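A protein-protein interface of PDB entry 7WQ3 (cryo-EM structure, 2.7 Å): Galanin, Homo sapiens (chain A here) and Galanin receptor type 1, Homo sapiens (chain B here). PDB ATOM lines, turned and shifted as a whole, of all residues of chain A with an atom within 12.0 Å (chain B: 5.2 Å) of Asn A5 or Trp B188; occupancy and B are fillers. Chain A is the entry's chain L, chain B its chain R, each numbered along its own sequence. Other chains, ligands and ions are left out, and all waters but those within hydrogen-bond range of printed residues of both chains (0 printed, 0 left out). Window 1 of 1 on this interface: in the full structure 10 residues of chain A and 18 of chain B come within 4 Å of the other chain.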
ATOM      1  N   GLY A   1      17.513  34.334   4.414  1.00  0.00           N
ATOM      2  CA  GLY A   1      17.850  33.150   5.181  1.00  0.00           C
ATOM      3  C   GLY A   1      18.957  32.323   4.554  1.00  0.00           C
ATOM      4  O   GLY A   1      19.196  31.183   4.954  1.00  0.00           O
ATOM      5  N   TRP A   2      19.636  32.900   3.564  1.00  0.00           N
ATOM      6  CA  TRP A   2      20.735  32.221   2.876  1.00  0.00           C
ATOM      7  C   TRP A   2      22.059  32.601   3.541  1.00  0.00           C
ATOM      8  O   TRP A   2      22.873  33.364   3.016  1.00  0.00           O
ATOM      9  CB  TRP A   2      20.727  32.563   1.392  1.00  0.00           C
ATOM     10  CG  TRP A   2      21.672  31.733   0.576  1.00  0.00           C
ATOM     11  CD1 TRP A   2      22.952  32.052   0.227  1.00  0.00           C
ATOM     12  CD2 TRP A   2      21.410  30.444   0.010  1.00  0.00           C
ATOM     13  NE1 TRP A   2      23.503  31.042  -0.522  1.00  0.00           N
ATOM     14  CE2 TRP A   2      22.578  30.042  -0.669  1.00  0.00           C
ATOM     15  CE3 TRP A   2      20.304  29.590   0.012  1.00  0.00           C
ATOM     16  CZ2 TRP A   2      22.669  28.825  -1.341  1.00  0.00           C
ATOM     17  CZ3 TRP A   2      20.396  28.382  -0.654  1.00  0.00           C
ATOM     18  CH2 TRP A   2      21.570  28.011  -1.321  1.00  0.00           C
ATOM     19  N   THR A   3      22.259  32.047   4.733  1.00  0.00           N
ATOM     20  CA  THR A   3      23.459  32.298   5.515  1.00  0.00           C
ATOM     21  C   THR A   3      24.566  31.335   5.084  1.00  0.00           C
ATOM     22  O   THR A   3      24.449  30.623   4.084  1.00  0.00           O
ATOM     23  CB  THR A   3      23.153  32.176   7.008  1.00  0.00           C
ATOM     24  OG1 THR A   3      24.348  32.411   7.764  1.00  0.00           O
ATOM     25  CG2 THR A   3      22.618  30.789   7.331  1.00  0.00           C
ATOM     26  N   LEU A   4      25.663  31.309   5.845  1.00  0.00           N
ATOM     27  CA  LEU A   4      26.775  30.425   5.510  1.00  0.00           C
ATOM     28  C   LEU A   4      26.427  28.967   5.784  1.00  0.00           C
ATOM     29  O   LEU A   4      26.956  28.063   5.126  1.00  0.00           O
ATOM     30  CB  LEU A   4      28.023  30.838   6.291  1.00  0.00           C
ATOM     31  CG  LEU A   4      29.317  30.072   6.007  1.00  0.00           C
ATOM     32  CD1 LEU A   4      29.742  30.250   4.557  1.00  0.00           C
ATOM     33  CD2 LEU A   4      30.422  30.517   6.952  1.00  0.00           C
ATOM     34  N   ASN A   5      25.533  28.719   6.745  1.00  0.00           N
ATOM     35  CA  ASN A   5      25.187  27.349   7.110  1.00  0.00           C
ATOM     36  C   ASN A   5      24.534  26.615   5.944  1.00  0.00           C
ATOM     37  O   ASN A   5      24.971  25.523   5.560  1.00  0.00           O
ATOM     38  CB  ASN A   5      24.268  27.351   8.332  1.00  0.00           C
ATOM     39  CG  ASN A   5      24.006  25.956   8.867  1.00  0.00           C
ATOM     40  OD1 ASN A   5      24.736  25.013   8.563  1.00  0.00           O
ATOM     41  ND2 ASN A   5      22.961  25.821   9.676  1.00  0.00           N
ATOM     42  N   SER A   6      23.485  27.201   5.363  1.00  0.00           N
ATOM     43  CA  SER A   6      22.800  26.561   4.244  1.00  0.00           C
ATOM     44  C   SER A   6      23.689  26.489   3.007  1.00  0.00           C
ATOM     45  O   SER A   6      23.652  25.496   2.270  1.00  0.00           O
ATOM     46  CB  SER A   6      21.503  27.305   3.927  1.00  0.00           C
ATOM     47  OG  SER A   6      21.761  28.659   3.598  1.00  0.00           O
ATOM     48  N   ALA A   7      24.490  27.529   2.765  1.00  0.00           N
ATOM     49  CA  ALA A   7      25.397  27.514   1.622  1.00  0.00           C
ATOM     50  C   ALA A   7      26.409  26.382   1.738  1.00  0.00           C
ATOM     51  O   ALA A   7      26.708  25.703   0.751  1.00  0.00           O
ATOM     52  CB  ALA A   7      26.107  28.861   1.497  1.00  0.00           C
ATOM     53  N   GLY A   8      26.942  26.159   2.941  1.00  0.00           N
ATOM     54  CA  GLY A   8      27.871  25.057   3.130  1.00  0.00           C
ATOM     55  C   GLY A   8      27.182  23.706   3.090  1.00  0.00           C
ATOM     56  O   GLY A   8      27.757  22.715   2.632  1.00  0.00           O
ATOM     57  N   TYR A   9      25.927  23.670   3.545  1.00  0.00           N
ATOM     58  CA  TYR A   9      25.139  22.409   3.543  1.00  0.00           C
ATOM     59  C   TYR A   9      24.863  21.996   2.098  1.00  0.00           C
ATOM     60  O   TYR A   9      24.842  20.783   1.815  1.00  0.00           O
ATOM     61  CB  TYR A   9      23.821  22.634   4.285  1.00  0.00           C
ATOM     62  CG  TYR A   9      23.002  21.399   4.554  1.00  0.00           C
ATOM     63  CD1 TYR A   9      23.549  20.307   5.204  1.00  0.00           C
ATOM     64  CD2 TYR A   9      21.674  21.327   4.167  1.00  0.00           C
ATOM     65  CE1 TYR A   9      22.798  19.172   5.455  1.00  0.00           C
ATOM     66  CE2 TYR A   9      20.909  20.200   4.413  1.00  0.00           C
ATOM     67  CZ  TYR A   9      21.474  19.117   5.060  1.00  0.00           C
ATOM     68  OH  TYR A   9      20.728  18.001   5.306  1.00  0.00           O
ATOM     69  N   LEU A  10      24.673  22.976   1.210  1.00  0.00           N
ATOM     70  CA  LEU A  10      24.341  22.679  -0.178  1.00  0.00           C
ATOM     71  C   LEU A  10      25.581  22.463  -1.040  1.00  0.00           C
ATOM     72  O   LEU A  10      25.648  21.492  -1.801  1.00  0.00           O
ATOM     73  CB  LEU A  10      23.482  23.803  -0.767  1.00  0.00           C
ATOM     74  CG  LEU A  10      23.101  23.634  -2.240  1.00  0.00           C
ATOM     75  CD1 LEU A  10      22.322  22.344  -2.452  1.00  0.00           C
ATOM     76  CD2 LEU A  10      22.303  24.830  -2.734  1.00  0.00           C
ATOM     77  N   LEU A  11      26.570  23.351  -0.936  1.00  0.00           N
ATOM     78  CA  LEU A  11      27.739  23.306  -1.802  1.00  0.00           C
ATOM     79  C   LEU A  11      28.927  22.581  -1.182  1.00  0.00           C
ATOM     80  O   LEU A  11      29.972  22.475  -1.833  1.00  0.00           O
ATOM     81  CB  LEU A  11      28.162  24.728  -2.188  1.00  0.00           C
ATOM     82  CG  LEU A  11      27.111  25.564  -2.918  1.00  0.00           C
ATOM     83  CD1 LEU A  11      27.659  26.937  -3.275  1.00  0.00           C
ATOM     84  CD2 LEU A  11      26.629  24.836  -4.161  1.00  0.00           C
ATOM     85  N   GLY A  12      28.799  22.084   0.044  1.00  0.00           N
ATOM     86  CA  GLY A  12      29.895  21.420   0.707  1.00  0.00           C
ATOM     87  C   GLY A  12      30.854  22.406   1.341  1.00  0.00           C
ATOM     88  O   GLY A  12      30.605  23.615   1.379  1.00  0.00           O
ATOM     89  N   PRO A  13      31.979  21.905   1.855  1.00  0.00           N
ATOM     90  CA  PRO A  13      32.960  22.795   2.491  1.00  0.00           C
ATOM     91  C   PRO A  13      33.823  23.539   1.482  1.00  0.00           C
ATOM     92  O   PRO A  13      35.052  23.554   1.601  1.00  0.00           O
ATOM     93  CB  PRO A  13      33.796  21.833   3.340  1.00  0.00           C
ATOM     94  CG  PRO A  13      33.750  20.554   2.573  1.00  0.00           C
ATOM     95  CD  PRO A  13      32.380  20.489   1.940  1.00  0.00           C
ATOM     96  N   HIS A  14      33.188  24.160   0.483  1.00  0.00           N
ATOM     97  CA  HIS A  14      33.921  24.912  -0.531  1.00  0.00           C
ATOM     98  C   HIS A  14      33.251  26.244  -0.856  1.00  0.00           C
ATOM     99  O   HIS A  14      33.624  26.887  -1.845  1.00  0.00           O
ATOM    100  CB  HIS A  14      34.078  24.089  -1.814  1.00  0.00           C
ATOM    101  CG  HIS A  14      35.034  22.943  -1.686  1.00  0.00           C
ATOM    102  ND1 HIS A  14      35.982  22.872  -0.688  1.00  0.00           N
ATOM    103  CD2 HIS A  14      35.188  21.823  -2.431  1.00  0.00           C
ATOM    104  CE1 HIS A  14      36.679  21.759  -0.824  1.00  0.00           C
ATOM    105  NE2 HIS A  14      36.217  21.104  -1.874  1.00  0.00           N
ATOM    106  N   ALA A  15      32.275  26.674  -0.055  1.00  0.00           N
ATOM    107  CA  ALA A  15      31.601  27.943  -0.302  1.00  0.00           C
ATOM    108  C   ALA A  15      32.375  29.138   0.235  1.00  0.00           C
ATOM    109  O   ALA A  15      32.023  30.277  -0.091  1.00  0.00           O
ATOM    110  CB  ALA A  15      30.199  27.920   0.311  1.00  0.00           C
ATOM    111  N   VAL A  16      33.410  28.914   1.039  1.00  0.00           N
ATOM    112  CA  VAL A  16      34.197  30.004   1.599  1.00  0.00           C
ATOM    113  C   VAL A  16      35.120  30.591   0.538  1.00  0.00           C
ATOM    114  O   VAL A  16      35.939  29.882  -0.047  1.00  0.00           O
ATOM    115  CB  VAL A  16      35.003  29.537   2.823  1.00  0.00           C
ATOM    116  CG1 VAL A  16      35.805  30.691   3.401  1.00  0.00           C
ATOM    117  CG2 VAL A  16      34.075  28.944   3.873  1.00  0.00           C
ATOM    118  N   THR B  94      16.461  23.204  11.513  1.00  0.00           N
ATOM    119  CA  THR B  94      17.483  23.833  12.344  1.00  0.00           C
ATOM    120  C   THR B  94      18.592  24.437  11.488  1.00  0.00           C
ATOM    121  O   THR B  94      19.215  25.433  11.877  1.00  0.00           O
ATOM    122  CB  THR B  94      18.057  22.813  13.329  1.00  0.00           C
ATOM    123  OG1 THR B  94      16.985  22.171  14.031  1.00  0.00           O
ATOM    124  CG2 THR B  94      18.975  23.489  14.338  1.00  0.00           C
ATOM    125  N   VAL B  95      18.847  23.850  10.316  1.00  0.00           N
ATOM    126  CA  VAL B  95      19.888  24.367   9.431  1.00  0.00           C
ATOM    127  C   VAL B  95      19.546  25.778   8.971  1.00  0.00           C
ATOM    128  O   VAL B  95      20.419  26.651   8.893  1.00  0.00           O
ATOM    129  CB  VAL B  95      20.094  23.415   8.238  1.00  0.00           C
ATOM    130  CG1 VAL B  95      21.208  23.924   7.335  1.00  0.00           C
ATOM    131  CG2 VAL B  95      20.398  22.008   8.728  1.00  0.00           C
ATOM    132  N   TYR B  96      18.273  26.027   8.665  1.00  0.00           N
ATOM    133  CA  TYR B  96      17.825  27.347   8.247  1.00  0.00           C
ATOM    134  C   TYR B  96      17.443  28.245   9.415  1.00  0.00           C
ATOM    135  O   TYR B  96      17.355  29.464   9.236  1.00  0.00           O
ATOM    136  CB  TYR B  96      16.634  27.222   7.289  1.00  0.00           C
ATOM    137  CG  TYR B  96      16.959  26.497   6.002  1.00  0.00           C
ATOM    138  CD1 TYR B  96      17.461  27.182   4.904  1.00  0.00           C
ATOM    139  CD2 TYR B  96      16.764  25.127   5.886  1.00  0.00           C
ATOM    140  CE1 TYR B  96      17.760  26.524   3.726  1.00  0.00           C
ATOM    141  CE2 TYR B  96      17.059  24.460   4.711  1.00  0.00           C
ATOM    142  CZ  TYR B  96      17.557  25.163   3.635  1.00  0.00           C
ATOM    143  OH  TYR B  96      17.853  24.505   2.464  1.00  0.00           O
ATOM    144  N   LEU B  98      18.963  27.938  12.946  1.00  0.00           N
ATOM    145  CA  LEU B  98      20.178  28.247  13.680  1.00  0.00           C
ATOM    146  C   LEU B  98      21.383  28.259  12.747  1.00  0.00           C
ATOM    147  O   LEU B  98      21.498  27.412  11.855  1.00  0.00           O
ATOM    148  CB  LEU B  98      20.411  27.224  14.796  1.00  0.00           C
ATOM    149  CG  LEU B  98      19.322  27.133  15.867  1.00  0.00           C
ATOM    150  CD1 LEU B  98      19.683  26.095  16.920  1.00  0.00           C
ATOM    151  CD2 LEU B  98      19.083  28.491  16.507  1.00  0.00           C
ATOM    152  N   PRO B  99      22.300  29.212  12.932  1.00  0.00           N
ATOM    153  CA  PRO B  99      23.478  29.295  12.060  1.00  0.00           C
ATOM    154  C   PRO B  99      24.590  28.321  12.413  1.00  0.00           C
ATOM    155  O   PRO B  99      25.648  28.363  11.774  1.00  0.00           O
ATOM    156  CB  PRO B  99      23.941  30.745  12.261  1.00  0.00           C
ATOM    157  CG  PRO B  99      23.540  31.058  13.659  1.00  0.00           C
ATOM    158  CD  PRO B  99      22.242  30.326  13.895  1.00  0.00           C
ATOM    159  N   THR B 100      24.392  27.449  13.400  1.00  0.00           N
ATOM    160  CA  THR B 100      25.421  26.498  13.796  1.00  0.00           C
ATOM    161  C   THR B 100      24.768  25.176  14.170  1.00  0.00           C
ATOM    162  O   THR B 100      23.618  25.147  14.617  1.00  0.00           O
ATOM    163  CB  THR B 100      26.257  27.027  14.970  1.00  0.00           C
ATOM    164  OG1 THR B 100      27.199  26.027  15.377  1.00  0.00           O
ATOM    165  CG2 THR B 100      25.361  27.386  16.147  1.00  0.00           C
ATOM    166  N   CYS B 108      24.334  14.134  13.647  1.00  0.00           N
ATOM    167  CA  CYS B 108      24.757  14.559  12.317  1.00  0.00           C
ATOM    168  C   CYS B 108      25.017  13.395  11.368  1.00  0.00           C
ATOM    169  O   CYS B 108      24.740  13.521  10.171  1.00  0.00           O
ATOM    170  CB  CYS B 108      26.016  15.427  12.427  1.00  0.00           C
ATOM    171  SG  CYS B 108      26.872  15.767  10.865  1.00  0.00           S
ATOM    172  N   HIS B 173      30.770   9.634   4.562  1.00  0.00           N
ATOM    173  CA  HIS B 173      31.357  10.954   4.355  1.00  0.00           C
ATOM    174  C   HIS B 173      30.790  12.009   5.303  1.00  0.00           C
ATOM    175  O   HIS B 173      31.552  12.777   5.899  1.00  0.00           O
ATOM    176  CB  HIS B 173      31.157  11.390   2.901  1.00  0.00           C
ATOM    177  CG  HIS B 173      31.779  10.465   1.901  1.00  0.00           C
ATOM    178  ND1 HIS B 173      31.176   9.293   1.496  1.00  0.00           N
ATOM    179  CD2 HIS B 173      32.953  10.535   1.231  1.00  0.00           C
ATOM    180  CE1 HIS B 173      31.951   8.684   0.617  1.00  0.00           C
ATOM    181  NE2 HIS B 173      33.035   9.417   0.438  1.00  0.00           N
ATOM    182  N   GLN B 174      29.456  12.081   5.387  1.00  0.00           N
ATOM    183  CA  GLN B 174      28.791  13.144   6.190  1.00  0.00           C
ATOM    184  C   GLN B 174      29.311  13.183   7.622  1.00  0.00           C
ATOM    185  O   GLN B 174      29.218  12.153   8.306  1.00  0.00           O
ATOM    186  CB  GLN B 174      27.272  12.987   6.193  1.00  0.00           C
ATOM    187  CG  GLN B 174      26.546  14.258   6.597  1.00  0.00           C
ATOM    188  CD  GLN B 174      26.054  15.029   5.398  1.00  0.00           C
ATOM    189  OE1 GLN B 174      25.995  16.256   5.404  1.00  0.00           O
ATOM    190  NE2 GLN B 174      25.672  14.304   4.359  1.00  0.00           N
ATOM    191  N   GLY B 175      29.811  14.339   8.054  1.00  0.00           N
ATOM    192  CA  GLY B 175      30.312  14.519   9.401  1.00  0.00           C
ATOM    193  C   GLY B 175      30.438  15.986   9.751  1.00  0.00           C
ATOM    194  O   GLY B 175      30.027  16.871   8.996  1.00  0.00           O
ATOM    195  N   LEU B 176      31.032  16.231  10.916  1.00  0.00           N
ATOM    196  CA  LEU B 176      31.206  17.591  11.398  1.00  0.00           C
ATOM    197  C   LEU B 176      32.378  18.275  10.703  1.00  0.00           C
ATOM    198  O   LEU B 176      33.294  17.629  10.187  1.00  0.00           O
ATOM    199  CB  LEU B 176      31.427  17.601  12.912  1.00  0.00           C
ATOM    200  CG  LEU B 176      30.235  17.202  13.781  1.00  0.00           C
ATOM    201  CD1 LEU B 176      30.548  17.444  15.249  1.00  0.00           C
ATOM    202  CD2 LEU B 176      28.987  17.963  13.362  1.00  0.00           C
ATOM    203  N   PHE B 177      32.334  19.605  10.696  1.00  0.00           N
ATOM    204  CA  PHE B 177      33.361  20.426  10.074  1.00  0.00           C
ATOM    205  C   PHE B 177      33.533  21.703  10.882  1.00  0.00           C
ATOM    206  O   PHE B 177      32.554  22.282  11.361  1.00  0.00           O
ATOM    207  CB  PHE B 177      33.008  20.763   8.618  1.00  0.00           C
ATOM    208  CG  PHE B 177      34.081  21.528   7.895  1.00  0.00           C
ATOM    209  CD1 PHE B 177      35.137  20.863   7.292  1.00  0.00           C
ATOM    210  CD2 PHE B 177      34.033  22.910   7.816  1.00  0.00           C
ATOM    211  CE1 PHE B 177      36.125  21.564   6.626  1.00  0.00           C
ATOM    212  CE2 PHE B 177      35.017  23.615   7.150  1.00  0.00           C
ATOM    213  CZ  PHE B 177      36.065  22.941   6.555  1.00  0.00           C
ATOM    214  N   PHE B 186      29.737  22.801  11.896  1.00  0.00           N
ATOM    215  CA  PHE B 186      28.679  22.526  10.935  1.00  0.00           C
ATOM    216  C   PHE B 186      28.630  21.030  10.668  1.00  0.00           C
ATOM    217  O   PHE B 186      29.560  20.289  10.990  1.00  0.00           O
ATOM    218  CB  PHE B 186      28.890  23.298   9.626  1.00  0.00           C
ATOM    219  CG  PHE B 186      28.918  24.790   9.793  1.00  0.00           C
ATOM    220  CD1 PHE B 186      27.748  25.529   9.728  1.00  0.00           C
ATOM    221  CD2 PHE B 186      30.114  25.455  10.006  1.00  0.00           C
ATOM    222  CE1 PHE B 186      27.771  26.903   9.879  1.00  0.00           C
ATOM    223  CE2 PHE B 186      30.143  26.827  10.158  1.00  0.00           C
ATOM    224  CZ  PHE B 186      28.970  27.553  10.094  1.00  0.00           C
ATOM    225  N   CYS B 187      27.530  20.590  10.064  1.00  0.00           N
ATOM    226  CA  CYS B 187      27.321  19.191   9.693  1.00  0.00           C
ATOM    227  C   CYS B 187      27.268  19.125   8.171  1.00  0.00           C
ATOM    228  O   CYS B 187      26.210  19.337   7.572  1.00  0.00           O
ATOM    229  CB  CYS B 187      26.045  18.642  10.328  1.00  0.00           C
ATOM    230  SG  CYS B 187      25.596  16.961   9.831  1.00  0.00           S
ATOM    231  N   TRP B 188      28.404  18.830   7.546  1.00  0.00           N
ATOM    232  CA  TRP B 188      28.537  18.882   6.096  1.00  0.00           C
ATOM    233  C   TRP B 188      28.982  17.523   5.562  1.00  0.00           C
ATOM    234  O   TRP B 188      29.255  16.588   6.317  1.00  0.00           O
ATOM    235  CB  TRP B 188      29.523  19.978   5.678  1.00  0.00           C
ATOM    236  CG  TRP B 188      29.035  21.370   5.948  1.00  0.00           C
ATOM    237  CD1 TRP B 188      27.766  21.743   6.283  1.00  0.00           C
ATOM    238  CD2 TRP B 188      29.810  22.574   5.911  1.00  0.00           C
ATOM    239  NE1 TRP B 188      27.702  23.105   6.453  1.00  0.00           N
ATOM    240  CE2 TRP B 188      28.944  23.639   6.229  1.00  0.00           C
ATOM    241  CE3 TRP B 188      31.152  22.856   5.636  1.00  0.00           C
ATOM    242  CZ2 TRP B 188      29.376  24.962   6.284  1.00  0.00           C
ATOM    243  CZ3 TRP B 188      31.578  24.172   5.689  1.00  0.00           C
ATOM    244  CH2 TRP B 188      30.692  25.208   6.011  1.00  0.00           C
ATOM    245  N   GLU B 189      29.057  17.425   4.233  1.00  0.00           N
ATOM    246  CA  GLU B 189      29.485  16.183   3.597  1.00  0.00           C
ATOM    247  C   GLU B 189      30.996  16.006   3.691  1.00  0.00           C
ATOM    248  O   GLU B 189      31.478  14.981   4.186  1.00  0.00           O
ATOM    249  CB  GLU B 189      29.031  16.152   2.136  1.00  0.00           C
ATOM    250  CG  GLU B 189      27.525  16.034   1.938  1.00  0.00           C
ATOM    251  CD  GLU B 189      26.794  17.344   2.162  1.00  0.00           C
ATOM    252  OE1 GLU B 189      27.465  18.389   2.298  1.00  0.00           O
ATOM    253  OE2 GLU B 189      25.546  17.329   2.201  1.00  0.00           O
ATOM    254  N   GLN B 190      31.753  16.997   3.219  1.00  0.00           N
ATOM    255  CA  GLN B 190      33.216  16.992   3.274  1.00  0.00           C
ATOM    256  C   GLN B 190      33.789  15.761   2.566  1.00  0.00           C
ATOM    257  O   GLN B 190      34.416  14.889   3.171  1.00  0.00           O
ATOM    258  CB  GLN B 190      33.710  17.084   4.724  1.00  0.00           C
ATOM    259  CG  GLN B 190      35.183  17.440   4.858  1.00  0.00           C
ATOM    260  CD  GLN B 190      35.636  17.515   6.301  1.00  0.00           C
ATOM    261  OE1 GLN B 190      34.851  17.293   7.223  1.00  0.00           O
ATOM    262  NE2 GLN B 190      36.910  17.830   6.506  1.00  0.00           N
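The backbone carbonyl oxygen (O) of Val B95 sits at hydrogen-bond distance from the side-chain amide nitrogen (ND2) of Asn A5. ND2 of Asn A5 sits at hydrogen-bond distance from O of Leu B98, 3.1 Å away. The indole nitrogen of Trp B188 sits close to the backbone NH of Tyr A9 (3.5 Å).
SG of Cys B108 is disulfide-bonded to SG of Cys B187, 2.0 Å away. The backbone carbonyl oxygen (O) of Trp B188 lies close to the side-chain amide oxygen (OE1) of Gln B174, at 3.4 Å. The side-chain amide oxygen of Gln B174 lies close to the side-chain carboxylate of Glu B189, 3.4 Å away. The backbone carbonyl oxygen (O) of Trp B188 sits at hydrogen-bond distance from the backbone NH (N) of Gly B175. The backbone carbonyl oxygen (O) of Leu B176 lies close to the side-chain amide oxygen (OE1) of Gln B190 (3.4 Å). O of Phe B186 sits at hydrogen-bond distance from N of Phe B177 (2.9 Å).
Among the printed residues, pairs that only touch across the chains: Asn A5 with Pro B99 (3.8 Å), Asn A5 with Phe B186 (3.3 Å), Asn A5 with Trp B188 (3.8 Å), Ser A6 with Tyr B96 (3.8 Å), Gly A8 with Trp B188 (3.5 Å), Tyr A9 with Cys B187 (3.7 Å), Tyr A9 with Glu B189 (3.5 Å), Pro A13 with Trp B188 (3.6 Å) and Pro A13 with Gln B190 (3.7 Å).
Of chain B, only Val B95, Leu B98, Pro B99, Phe B186 and Trp B188 come within 4 Å of Asn A5. Printed residues of chain B within 4 Å of Tyr A9: Cys B187 (3.7 Å), Trp B188 (3.5 Å) and Glu B189 (3.5 Å). Printed residues of chain B within 4 Å of Pro A13: Trp B188 (3.6 Å) and Gln B190 (3.7 Å). Val A16 touches none of the printed residues of chain B. Val B95 touches just one residue of chain A: Asn A5 (2.8 Å). Tyr B96 touches just one residue of chain A: Ser A6. Of the printed residues of chain A, Leu B98 touches Asn A5 (3.1 Å). Pro B99 touches one residue of chain A. No residue of chain A comes within 4 Å of Thr B100. No residue of chain A comes within 4 Å of Gln B174. No residue of chain A comes within 4 Å of Gly B175. Leu B176 touches none of the printed residues of chain A. Printed residues of chain A within 4 Å of Phe B186: Asn A5 (3.3 Å). Of the printed residues of chain A, Cys B187 touches Tyr A9 (3.7 Å). Trp B188 touches four residues of chain A. Glu B189 touches just one residue of chain A: Tyr A9. The nearest residue of chain B that does not touch Asn A5 is Thr B100 (4.3 Å). The nearest residue of chain A that does not touch Trp B188 is Leu A4 (4.1 Å). The nearest printed residue of chain B that does not touch Pro A13 is Phe B177 (4.04 Å).
Along chain A the printed residues that touch a printed residue of chain B span positions 5 to 13. Among the printed residues, no Asp or Glu carboxylate lies within 4 Å of a Lys or Arg side-chain nitrogen of the other chain.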
